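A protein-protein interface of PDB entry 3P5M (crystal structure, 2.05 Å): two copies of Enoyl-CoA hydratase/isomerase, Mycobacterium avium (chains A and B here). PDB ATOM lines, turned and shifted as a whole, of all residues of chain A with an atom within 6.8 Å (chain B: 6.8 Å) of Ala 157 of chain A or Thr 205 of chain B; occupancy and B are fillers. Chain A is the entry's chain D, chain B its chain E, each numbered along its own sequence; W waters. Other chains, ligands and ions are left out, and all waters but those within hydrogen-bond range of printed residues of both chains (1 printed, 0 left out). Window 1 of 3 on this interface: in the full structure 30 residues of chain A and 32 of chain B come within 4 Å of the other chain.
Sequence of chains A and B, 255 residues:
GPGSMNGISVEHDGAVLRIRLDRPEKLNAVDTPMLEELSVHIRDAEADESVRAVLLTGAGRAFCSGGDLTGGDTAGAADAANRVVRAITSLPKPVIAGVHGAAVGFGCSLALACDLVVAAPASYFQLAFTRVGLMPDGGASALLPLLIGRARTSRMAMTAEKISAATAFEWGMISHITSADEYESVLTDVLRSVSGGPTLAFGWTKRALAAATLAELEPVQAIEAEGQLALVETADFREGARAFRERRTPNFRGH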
ATOM      1  N   LEU A 127     -36.018 -10.872  19.937  1.00  0.00           N
ATOM      2  CA  LEU A 127     -34.826 -11.633  19.594  1.00  0.00           C
ATOM      3  C   LEU A 127     -35.015 -12.994  20.246  1.00  0.00           C
ATOM      4  O   LEU A 127     -34.543 -13.238  21.366  1.00  0.00           O
ATOM      5  CB  LEU A 127     -33.578 -10.923  20.152  1.00  0.00           C
ATOM      6  CG  LEU A 127     -33.297  -9.489  19.628  1.00  0.00           C
ATOM      7  CD1 LEU A 127     -32.066  -8.920  20.299  1.00  0.00           C
ATOM      8  CD2 LEU A 127     -33.109  -9.478  18.149  1.00  0.00           C
ATOM      9  N   ALA A 128     -35.737 -13.856  19.558  1.00  0.00           N
ATOM     10  CA  ALA A 128     -36.164 -15.117  20.150  1.00  0.00           C
ATOM     11  C   ALA A 128     -35.088 -16.170  20.021  1.00  0.00           C
ATOM     12  O   ALA A 128     -35.305 -17.287  20.475  1.00  0.00           O
ATOM     13  CB  ALA A 128     -37.470 -15.620  19.506  1.00  0.00           C
ATOM     14  N   PHE A 129     -33.936 -15.804  19.453  1.00  0.00           N
ATOM     15  CA  PHE A 129     -32.843 -16.755  19.095  1.00  0.00           C
ATOM     16  C   PHE A 129     -32.387 -17.645  20.257  1.00  0.00           C
ATOM     17  O   PHE A 129     -32.134 -18.829  20.082  1.00  0.00           O
ATOM     18  CB  PHE A 129     -31.576 -16.012  18.625  1.00  0.00           C
ATOM     19  CG  PHE A 129     -31.806 -15.025  17.499  1.00  0.00           C
ATOM     20  CD1 PHE A 129     -31.681 -15.419  16.161  1.00  0.00           C
ATOM     21  CD2 PHE A 129     -32.141 -13.699  17.779  1.00  0.00           C
ATOM     22  CE1 PHE A 129     -31.890 -14.507  15.131  1.00  0.00           C
ATOM     23  CE2 PHE A 129     -32.302 -12.782  16.747  1.00  0.00           C
ATOM     24  CZ  PHE A 129     -32.173 -13.194  15.421  1.00  0.00           C
ATOM     25  N   THR A 130     -32.227 -17.048  21.431  1.00  0.00           N
ATOM     26  CA  THR A 130     -31.692 -17.788  22.586  1.00  0.00           C
ATOM     27  C   THR A 130     -32.684 -18.796  23.147  1.00  0.00           C
ATOM     28  O   THR A 130     -32.303 -19.701  23.878  1.00  0.00           O
ATOM     29  CB  THR A 130     -31.181 -16.836  23.738  1.00  0.00           C
ATOM     30  OG1 THR A 130     -32.244 -15.963  24.119  1.00  0.00           O
ATOM     31  CG2 THR A 130     -29.956 -16.044  23.279  1.00  0.00           C
ATOM     32  N   ARG A 131     -33.967 -18.627  22.842  1.00  0.00           N
ATOM     33  CA  ARG A 131     -34.959 -19.651  23.234  1.00  0.00           C
ATOM     34  C   ARG A 131     -34.672 -20.993  22.571  1.00  0.00           C
ATOM     35  O   ARG A 131     -35.122 -22.044  23.064  1.00  0.00           O
ATOM     36  CB  ARG A 131     -36.416 -19.222  22.947  1.00  0.00           C
ATOM     37  CG  ARG A 131     -36.866 -17.985  23.741  1.00  0.00           C
ATOM     38  CD  ARG A 131     -38.396 -17.911  23.870  1.00  0.00           C
ATOM     39  NE  ARG A 131     -38.889 -16.718  24.582  1.00  0.00           N
ATOM     40  CZ  ARG A 131     -38.681 -16.452  25.875  1.00  0.00           C
ATOM     41  NH1 ARG A 131     -37.947 -17.263  26.623  1.00  0.00           N
ATOM     42  NH2 ARG A 131     -39.184 -15.358  26.424  1.00  0.00           N
ATOM     43  N   LEU A 134     -29.517 -20.129  20.126  1.00  0.00           N
ATOM     44  CA  LEU A 134     -28.756 -19.425  19.078  1.00  0.00           C
ATOM     45  C   LEU A 134     -28.562 -17.968  19.458  1.00  0.00           C
ATOM     46  O   LEU A 134     -29.154 -17.505  20.447  1.00  0.00           O
ATOM     47  CB  LEU A 134     -29.477 -19.513  17.721  1.00  0.00           C
ATOM     48  CG  LEU A 134     -29.681 -20.955  17.174  1.00  0.00           C
ATOM     49  CD1 LEU A 134     -30.470 -20.971  15.846  1.00  0.00           C
ATOM     50  CD2 LEU A 134     -28.355 -21.761  17.032  1.00  0.00           C
ATOM     51  N   MET A 135     -27.786 -17.239  18.650  1.00  0.00           N
ATOM     52  CA  MET A 135     -27.518 -15.838  18.922  1.00  0.00           C
ATOM     53  C   MET A 135     -28.171 -14.949  17.853  1.00  0.00           C
ATOM     54  O   MET A 135     -28.628 -15.462  16.804  1.00  0.00           O
ATOM     55  CB  MET A 135     -26.012 -15.635  18.944  1.00  0.00           C
ATOM     56  CG  MET A 135     -25.393 -15.785  17.545  1.00  0.00           C
ATOM     57  SD  MET A 135     -23.650 -15.395  17.520  1.00  0.00           S
ATOM     58  CE  MET A 135     -23.725 -13.682  18.133  1.00  0.00           C
ATOM     59  N   PRO A 136     -28.199 -13.617  18.089  1.00  0.00           N
ATOM     60  CA  PRO A 136     -28.775 -12.701  17.087  1.00  0.00           C
ATOM     61  C   PRO A 136     -28.039 -12.759  15.768  1.00  0.00           C
ATOM     62  O   PRO A 136     -26.895 -13.107  15.746  1.00  0.00           O
ATOM     63  CB  PRO A 136     -28.595 -11.325  17.746  1.00  0.00           C
ATOM     64  CG  PRO A 136     -28.766 -11.626  19.238  1.00  0.00           C
ATOM     65  CD  PRO A 136     -27.937 -12.911  19.376  1.00  0.00           C
ATOM     66  N   SER A 141     -26.949  -7.337  16.305  1.00  0.00           N
ATOM     67  CA  SER A 141     -26.087  -6.938  17.421  1.00  0.00           C
ATOM     68  C   SER A 141     -25.476  -5.542  17.175  1.00  0.00           C
ATOM     69  O   SER A 141     -25.153  -4.856  18.150  1.00  0.00           O
ATOM     70  CB  SER A 141     -24.959  -7.944  17.680  1.00  0.00           C
ATOM     71  OG  SER A 141     -25.463  -9.253  17.750  1.00  0.00           O
ATOM     72  N   LEU A 144     -29.229  -2.746  16.929  1.00  0.00           N
ATOM     73  CA  LEU A 144     -30.010  -2.412  18.101  1.00  0.00           C
ATOM     74  C   LEU A 144     -29.314  -1.411  19.094  1.00  0.00           C
ATOM     75  O   LEU A 144     -29.970  -0.503  19.626  1.00  0.00           O
ATOM     76  CB  LEU A 144     -30.541  -3.695  18.760  1.00  0.00           C
ATOM     77  CG  LEU A 144     -31.837  -4.253  18.151  1.00  0.00           C
ATOM     78  CD1 LEU A 144     -32.125  -5.695  18.520  1.00  0.00           C
ATOM     79  CD2 LEU A 144     -33.005  -3.382  18.622  1.00  0.00           C
ATOM     80  N   ARG A 152     -30.619  -2.204  26.900  1.00  0.00           N
ATOM     81  CA  ARG A 152     -31.884  -2.737  26.399  1.00  0.00           C
ATOM     82  C   ARG A 152     -31.659  -3.845  25.360  1.00  0.00           C
ATOM     83  O   ARG A 152     -32.459  -4.817  25.277  1.00  0.00           O
ATOM     84  CB  ARG A 152     -32.785  -1.627  25.807  1.00  0.00           C
ATOM     85  CG  ARG A 152     -33.480  -0.816  26.894  1.00  0.00           C
ATOM     86  CD  ARG A 152     -33.989   0.535  26.383  1.00  0.00           C
ATOM     87  NE  ARG A 152     -34.912   1.050  27.387  1.00  0.00           N
ATOM     88  CZ  ARG A 152     -35.271   2.315  27.581  1.00  0.00           C
ATOM     89  NH1 ARG A 152     -36.121   2.604  28.587  1.00  0.00           N
ATOM     90  NH2 ARG A 152     -34.799   3.271  26.820  1.00  0.00           N
ATOM     91  N   THR A 153     -30.589  -3.691  24.560  1.00  0.00           N
ATOM     92  CA  THR A 153     -30.211  -4.732  23.604  1.00  0.00           C
ATOM     93  C   THR A 153     -29.785  -6.039  24.338  1.00  0.00           C
ATOM     94  O   THR A 153     -30.274  -7.122  24.012  1.00  0.00           O
ATOM     95  CB  THR A 153     -29.101  -4.266  22.638  1.00  0.00           C
ATOM     96  OG1 THR A 153     -29.533  -3.096  21.960  1.00  0.00           O
ATOM     97  CG2 THR A 153     -28.764  -5.364  21.616  1.00  0.00           C
ATOM     98  N   SER A 154     -28.875  -5.918  25.314  1.00  0.00           N
ATOM     99  CA  SER A 154     -28.448  -7.082  26.071  1.00  0.00           C
ATOM    100  C   SER A 154     -29.668  -7.794  26.634  1.00  0.00           C
ATOM    101  O   SER A 154     -29.784  -9.029  26.511  1.00  0.00           O
ATOM    102  CB  SER A 154     -27.494  -6.676  27.185  1.00  0.00           C
ATOM    103  OG  SER A 154     -26.247  -6.309  26.634  1.00  0.00           O
ATOM    104  N   ARG A 155     -30.587  -7.013  27.230  1.00  0.00           N
ATOM    105  CA  ARG A 155     -31.829  -7.556  27.730  1.00  0.00           C
ATOM    106  C   ARG A 155     -32.636  -8.310  26.659  1.00  0.00           C
ATOM    107  O   ARG A 155     -33.046  -9.450  26.888  1.00  0.00           O
ATOM    108  CB  ARG A 155     -32.732  -6.493  28.395  1.00  0.00           C
ATOM    109  CG  ARG A 155     -33.878  -7.197  29.237  1.00  0.00           C
ATOM    110  CD  ARG A 155     -34.691  -6.253  30.138  1.00  0.00           C
ATOM    111  NE  ARG A 155     -35.948  -6.898  30.481  1.00  0.00           N
ATOM    112  CZ  ARG A 155     -36.773  -6.528  31.463  1.00  0.00           C
ATOM    113  NH1 ARG A 155     -36.479  -5.500  32.255  1.00  0.00           N
ATOM    114  NH2 ARG A 155     -37.891  -7.225  31.676  1.00  0.00           N
ATOM    115  N   MET A 156     -32.882  -7.689  25.510  1.00  0.00           N
ATOM    116  CA  MET A 156     -33.681  -8.357  24.478  1.00  0.00           C
ATOM    117  C   MET A 156     -33.052  -9.663  24.066  1.00  0.00           C
ATOM    118  O   MET A 156     -33.735 -10.640  23.837  1.00  0.00           O
ATOM    119  CB  MET A 156     -33.834  -7.465  23.236  1.00  0.00           C
ATOM    120  CG  MET A 156     -34.811  -6.318  23.415  1.00  0.00           C
ATOM    121  SD  MET A 156     -34.841  -5.301  21.893  1.00  0.00           S
ATOM    122  CE  MET A 156     -35.786  -6.410  20.792  1.00  0.00           C
ATOM    123  N   ALA A 157     -31.726  -9.664  23.957  1.00  0.00           N
ATOM    124  CA  ALA A 157     -31.002 -10.798  23.416  1.00  0.00           C
ATOM    125  C   ALA A 157     -30.962 -11.932  24.413  1.00  0.00           C
ATOM    126  O   ALA A 157     -31.192 -13.112  24.044  1.00  0.00           O
ATOM    127  CB  ALA A 157     -29.542 -10.385  23.032  1.00  0.00           C
ATOM    128  N   MET A 158     -30.659 -11.574  25.666  1.00  0.00           N
ATOM    129  CA  MET A 158     -30.473 -12.554  26.698  1.00  0.00           C
ATOM    130  C   MET A 158     -31.765 -13.117  27.301  1.00  0.00           C
ATOM    131  O   MET A 158     -31.770 -14.257  27.713  1.00  0.00           O
ATOM    132  CB  MET A 158     -29.530 -12.051  27.775  1.00  0.00           C
ATOM    133  CG  MET A 158     -28.070 -12.085  27.321  1.00  0.00           C
ATOM    134  SD  MET A 158     -27.082 -11.446  28.645  1.00  0.00           S
ATOM    135  CE  MET A 158     -25.453 -11.496  27.865  1.00  0.00           C
ATOM    136  N   THR A 159     -32.854 -12.341  27.315  1.00  0.00           N
ATOM    137  CA  THR A 159     -34.144 -12.828  27.845  1.00  0.00           C
ATOM    138  C   THR A 159     -35.129 -13.269  26.760  1.00  0.00           C
ATOM    139  O   THR A 159     -36.107 -13.963  27.059  1.00  0.00           O
ATOM    140  CB  THR A 159     -34.854 -11.730  28.636  1.00  0.00           C
ATOM    141  OG1 THR A 159     -35.333 -10.739  27.702  1.00  0.00           O
ATOM    142  CG2 THR A 159     -33.912 -11.130  29.641  1.00  0.00           C
ATOM    143  N   ALA A 160     -34.870 -12.860  25.510  1.00  0.00           N
ATOM    144  CA  ALA A 160     -35.767 -13.143  24.388  1.00  0.00           C
ATOM    145  C   ALA A 160     -37.226 -12.776  24.664  1.00  0.00           C
ATOM    146  O   ALA A 160     -38.147 -13.497  24.254  1.00  0.00           O
ATOM    147  CB  ALA A 160     -35.668 -14.620  23.947  1.00  0.00           C
ATOM    148  N   GLU A 161     -37.424 -11.670  25.351  1.00  0.00           N
ATOM    149  CA  GLU A 161     -38.748 -11.122  25.623  1.00  0.00           C
ATOM    150  C   GLU A 161     -39.312 -10.384  24.415  1.00  0.00           C
ATOM    151  O   GLU A 161     -38.566  -9.779  23.596  1.00  0.00           O
ATOM    152  CB  GLU A 161     -38.686 -10.141  26.816  1.00  0.00           C
ATOM    153  CG  GLU A 161     -38.546 -10.837  28.155  1.00  0.00           C
ATOM    154  CD  GLU A 161     -38.003  -9.929  29.312  1.00  0.00           C
ATOM    155  OE1 GLU A 161     -37.969  -8.683  29.175  1.00  0.00           O
ATOM    156  OE2 GLU A 161     -37.596 -10.493  30.360  1.00  0.00           O
ATOM    157  N   LEU A 231     -22.729 -22.449  17.316  1.00  0.00           N
ATOM    158  CA  LEU A 231     -23.867 -22.791  18.172  1.00  0.00           C
ATOM    159  C   LEU A 231     -24.750 -23.931  17.646  1.00  0.00           C
ATOM    160  O   LEU A 231     -25.334 -24.665  18.451  1.00  0.00           O
ATOM    161  CB  LEU A 231     -24.725 -21.564  18.483  1.00  0.00           C
ATOM    162  CG  LEU A 231     -23.993 -20.474  19.310  1.00  0.00           C
ATOM    163  CD1 LEU A 231     -24.813 -19.169  19.341  1.00  0.00           C
ATOM    164  CD2 LEU A 231     -23.649 -20.909  20.775  1.00  0.00           C
ATOM    165  N   LEU B 200     -23.413 -20.715  26.132  1.00  0.00           N
ATOM    166  CA  LEU B 200     -22.565 -20.464  24.969  1.00  0.00           C
ATOM    167  C   LEU B 200     -23.186 -19.456  23.998  1.00  0.00           C
ATOM    168  O   LEU B 200     -22.471 -18.611  23.467  1.00  0.00           O
ATOM    169  CB  LEU B 200     -22.181 -21.752  24.231  1.00  0.00           C
ATOM    170  CG  LEU B 200     -21.395 -22.805  25.007  1.00  0.00           C
ATOM    171  CD1 LEU B 200     -21.203 -24.065  24.113  1.00  0.00           C
ATOM    172  CD2 LEU B 200     -20.036 -22.280  25.574  1.00  0.00           C
ATOM    173  N   ALA B 201     -24.505 -19.529  23.780  1.00  0.00           N
ATOM    174  CA  ALA B 201     -25.208 -18.506  22.991  1.00  0.00           C
ATOM    175  C   ALA B 201     -25.015 -17.097  23.606  1.00  0.00           C
ATOM    176  O   ALA B 201     -24.801 -16.122  22.889  1.00  0.00           O
ATOM    177  CB  ALA B 201     -26.717 -18.851  22.881  1.00  0.00           C
ATOM    178  N   PHE B 202     -25.080 -17.022  24.926  1.00  0.00           N
ATOM    179  CA  PHE B 202     -24.865 -15.764  25.644  1.00  0.00           C
ATOM    180  C   PHE B 202     -23.430 -15.259  25.457  1.00  0.00           C
ATOM    181  O   PHE B 202     -23.225 -14.081  25.215  1.00  0.00           O
ATOM    182  CB  PHE B 202     -25.120 -15.932  27.137  1.00  0.00           C
ATOM    183  CG  PHE B 202     -26.565 -16.153  27.502  1.00  0.00           C
ATOM    184  CD1 PHE B 202     -27.610 -15.752  26.642  1.00  0.00           C
ATOM    185  CD2 PHE B 202     -26.879 -16.755  28.714  1.00  0.00           C
ATOM    186  CE1 PHE B 202     -28.931 -15.977  26.986  1.00  0.00           C
ATOM    187  CE2 PHE B 202     -28.218 -16.984  29.086  1.00  0.00           C
ATOM    188  CZ  PHE B 202     -29.255 -16.591  28.230  1.00  0.00           C
ATOM    189  N   GLY B 203     -22.456 -16.161  25.564  1.00  0.00           N
ATOM    190  CA  GLY B 203     -21.062 -15.823  25.318  1.00  0.00           C
ATOM    191  C   GLY B 203     -20.878 -15.209  23.926  1.00  0.00           C
ATOM    192  O   GLY B 203     -20.271 -14.141  23.809  1.00  0.00           O
ATOM    193  N   TRP B 204     -21.382 -15.885  22.874  1.00  0.00           N
ATOM    194  CA  TRP B 204     -21.332 -15.325  21.513  1.00  0.00           C
ATOM    195  C   TRP B 204     -22.081 -14.005  21.333  1.00  0.00           C
ATOM    196  O   TRP B 204     -21.544 -13.073  20.743  1.00  0.00           O
ATOM    197  CB  TRP B 204     -21.792 -16.358  20.483  1.00  0.00           C
ATOM    198  CG  TRP B 204     -20.681 -17.292  20.090  1.00  0.00           C
ATOM    199  CD1 TRP B 204     -20.515 -18.564  20.499  1.00  0.00           C
ATOM    200  CD2 TRP B 204     -19.586 -16.995  19.246  1.00  0.00           C
ATOM    201  NE1 TRP B 204     -19.392 -19.108  19.948  1.00  0.00           N
ATOM    202  CE2 TRP B 204     -18.797 -18.168  19.157  1.00  0.00           C
ATOM    203  CE3 TRP B 204     -19.216 -15.878  18.505  1.00  0.00           C
ATOM    204  CZ2 TRP B 204     -17.633 -18.238  18.399  1.00  0.00           C
ATOM    205  CZ3 TRP B 204     -18.059 -15.954  17.730  1.00  0.00           C
ATOM    206  CH2 TRP B 204     -17.292 -17.124  17.675  1.00  0.00           C
ATOM    207  N   THR B 205     -23.312 -13.929  21.843  1.00  0.00           N
ATOM    208  CA  THR B 205     -24.086 -12.670  21.882  1.00  0.00           C
ATOM    209  C   THR B 205     -23.261 -11.530  22.467  1.00  0.00           C
ATOM    210  O   THR B 205     -23.188 -10.433  21.859  1.00  0.00           O
ATOM    211  CB  THR B 205     -25.382 -12.848  22.720  1.00  0.00           C
ATOM    212  OG1 THR B 205     -26.194 -13.853  22.113  1.00  0.00           O
ATOM    213  CG2 THR B 205     -26.177 -11.515  22.903  1.00  0.00           C
ATOM    214  N   LYS B 206     -22.623 -11.783  23.619  1.00  0.00           N
ATOM    215  CA  LYS B 206     -21.750 -10.785  24.261  1.00  0.00           C
ATOM    216  C   LYS B 206     -20.630 -10.337  23.351  1.00  0.00           C
ATOM    217  O   LYS B 206     -20.328  -9.136  23.251  1.00  0.00           O
ATOM    218  CB  LYS B 206     -21.111 -11.312  25.549  1.00  0.00           C
ATOM    219  CG  LYS B 206     -21.976 -11.223  26.767  1.00  0.00           C
ATOM    220  CD  LYS B 206     -21.235 -11.571  28.072  1.00  0.00           C
ATOM    221  CE  LYS B 206     -20.167 -10.512  28.488  1.00  0.00           C
ATOM    222  NZ  LYS B 206     -19.881 -10.620  29.980  1.00  0.00           N
ATOM    223  N   ARG B 207     -19.988 -11.302  22.695  1.00  0.00           N
ATOM    224  CA  ARG B 207     -18.856 -10.975  21.831  1.00  0.00           C
ATOM    225  C   ARG B 207     -19.289 -10.026  20.711  1.00  0.00           C
ATOM    226  O   ARG B 207     -18.574  -9.066  20.405  1.00  0.00           O
ATOM    227  CB  ARG B 207     -18.175 -12.247  21.297  1.00  0.00           C
ATOM    228  CG  ARG B 207     -17.221 -12.081  20.087  1.00  0.00           C
ATOM    229  CD  ARG B 207     -15.847 -11.439  20.404  1.00  0.00           C
ATOM    230  NE  ARG B 207     -15.036 -11.340  19.179  1.00  0.00           N
ATOM    231  CZ  ARG B 207     -14.110 -10.415  18.929  1.00  0.00           C
ATOM    232  NH1 ARG B 207     -13.834  -9.480  19.819  1.00  0.00           N
ATOM    233  NH2 ARG B 207     -13.456 -10.432  17.770  1.00  0.00           N
ATOM    234  N   ALA B 208     -20.459 -10.281  20.124  1.00  0.00           N
ATOM    235  CA  ALA B 208     -20.977  -9.478  19.024  1.00  0.00           C
ATOM    236  C   ALA B 208     -21.375  -8.082  19.503  1.00  0.00           C
ATOM    237  O   ALA B 208     -21.039  -7.077  18.854  1.00  0.00           O
ATOM    238  CB  ALA B 208     -22.189 -10.181  18.365  1.00  0.00           C
ATOM    239  N   LEU B 209     -22.107  -8.030  20.618  1.00  0.00           N
ATOM    240  CA  LEU B 209     -22.451  -6.764  21.250  1.00  0.00           C
ATOM    241  C   LEU B 209     -21.194  -5.927  21.596  1.00  0.00           C
ATOM    242  O   LEU B 209     -21.157  -4.715  21.314  1.00  0.00           O
ATOM    243  CB  LEU B 209     -23.293  -6.996  22.522  1.00  0.00           C
ATOM    244  CG  LEU B 209     -24.729  -7.396  22.189  1.00  0.00           C
ATOM    245  CD1 LEU B 209     -25.572  -7.713  23.448  1.00  0.00           C
ATOM    246  CD2 LEU B 209     -25.391  -6.285  21.346  1.00  0.00           C
ATOM    247  N   ALA B 210     -20.178  -6.586  22.171  1.00  0.00           N
ATOM    248  CA  ALA B 210     -18.902  -5.943  22.480  1.00  0.00           C
ATOM    249  C   ALA B 210     -18.201  -5.328  21.253  1.00  0.00           C
ATOM    250  O   ALA B 210     -17.741  -4.197  21.321  1.00  0.00           O
ATOM    251  CB  ALA B 210     -17.938  -6.926  23.226  1.00  0.00           C
HETATM  252  O   HOH W   1     -25.671 -10.294  20.211  1.00  0.00           O
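No position is printed for both chains.
Of the printed residues of chain B, Leu 134 of chain A touches Ala 201 (3.7 Å). Printed residues of chain B within 4 Å of Met 135 of chain A: Trp 204, Thr 205 and Ala 208. Printed residues of chain B within 4 Å of Ser 141 of chain A: Ala 208 and Leu 209. Leu 144 of chain A touches none of the printed residues of chain B. Of the printed residues of chain B, Thr 153 of chain A touches Leu 209 (3.5 Å). Ala 157 of chain A touches one residue of chain B. Glu 161 of chain A touches none of the printed residues of chain B. The nearest residue of chain B that does not touch Ala 157 of chain A is Phe 202 of chain B (4.7 Å). The nearest residue of chain A that does not touch Thr 205 of chain B is Thr 130 of chain A (4.5 Å). The nearest printed residue of chain B that does not touch Leu 231 of chain A is Phe 202 of chain B (5.9 Å).
The backbone carbonyl oxygen (O) of Ala 201 of chain B is in hydrogen-bond range of the side-chain hydroxyl (OG1) of Thr 205 of chain B (2.8 Å). N of Leu 134 of chain A is in hydrogen-bond range of O of Phe 129 of chain A. O of Ala 157 of chain A lies within hydrogen-bond range of OG1 of Thr 130 of chain A.
Among the printed residues, pairs that only touch across the chains: Pro 136 of chain A with Thr 205 of chain B (3.4 Å), Met 158 of chain A with Phe 202 of chain B (3.4 Å), Leu 231 of chain A with Ala 201 of chain B (3.4 Å), Met 135 of chain A with Trp 204 of chain B (3.5 Å), Ser 141 of chain A with Ala 208 of chain B (3.5 Å), Thr 153 of chain A with Leu 209 of chain B (3.5 Å), Ser 141 of chain A with Leu 209 of chain B (3.5 Å), Ser 154 of chain A with Leu 209 of chain B (3.5 Å), Ala 157 of chain A with Thr 205 of chain B (3.6 Å), Leu 231 of chain A with Leu 200 of chain B (3.6 Å), Met 135 of chain A with Thr 205 of chain B (3.6 Å), Met 158 of chain A with Lys 206 of chain B (3.7 Å), Leu 134 of chain A with Ala 201 of chain B (3.7 Å), Met 135 of chain A with Ala 208 of chain B (3.8 Å), Thr 130 of chain A with Phe 202 of chain B (3.8 Å) and Leu 231 of chain A with Trp 204 of chain B (3.9 Å).
Water W1 lies within hydrogen-bond range of the side-chain hydroxyl of Ser 141 of chain A (2.7 Å) and the backbone carbonyl oxygen of Thr 205 of chain B (3.0 Å).
Hydrophobic or aromatic side chains of chain B that line the printed part of chain A: Leu 200, Ala 201, Phe 202, Trp 204, Ala 208 and Leu 209. Of the 21 printed residues of chain A, 10 touch a printed residue of chain B. Hydrophobic or aromatic side chains of chain A that line the printed part of chain B: Met 135, Pro 136, Ala 157, Met 158 and Leu 231. Among the printed residues, no Asp or Glu carboxylate lies within 4 Å of a Lys or Arg side-chain nitrogen of the other chain.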
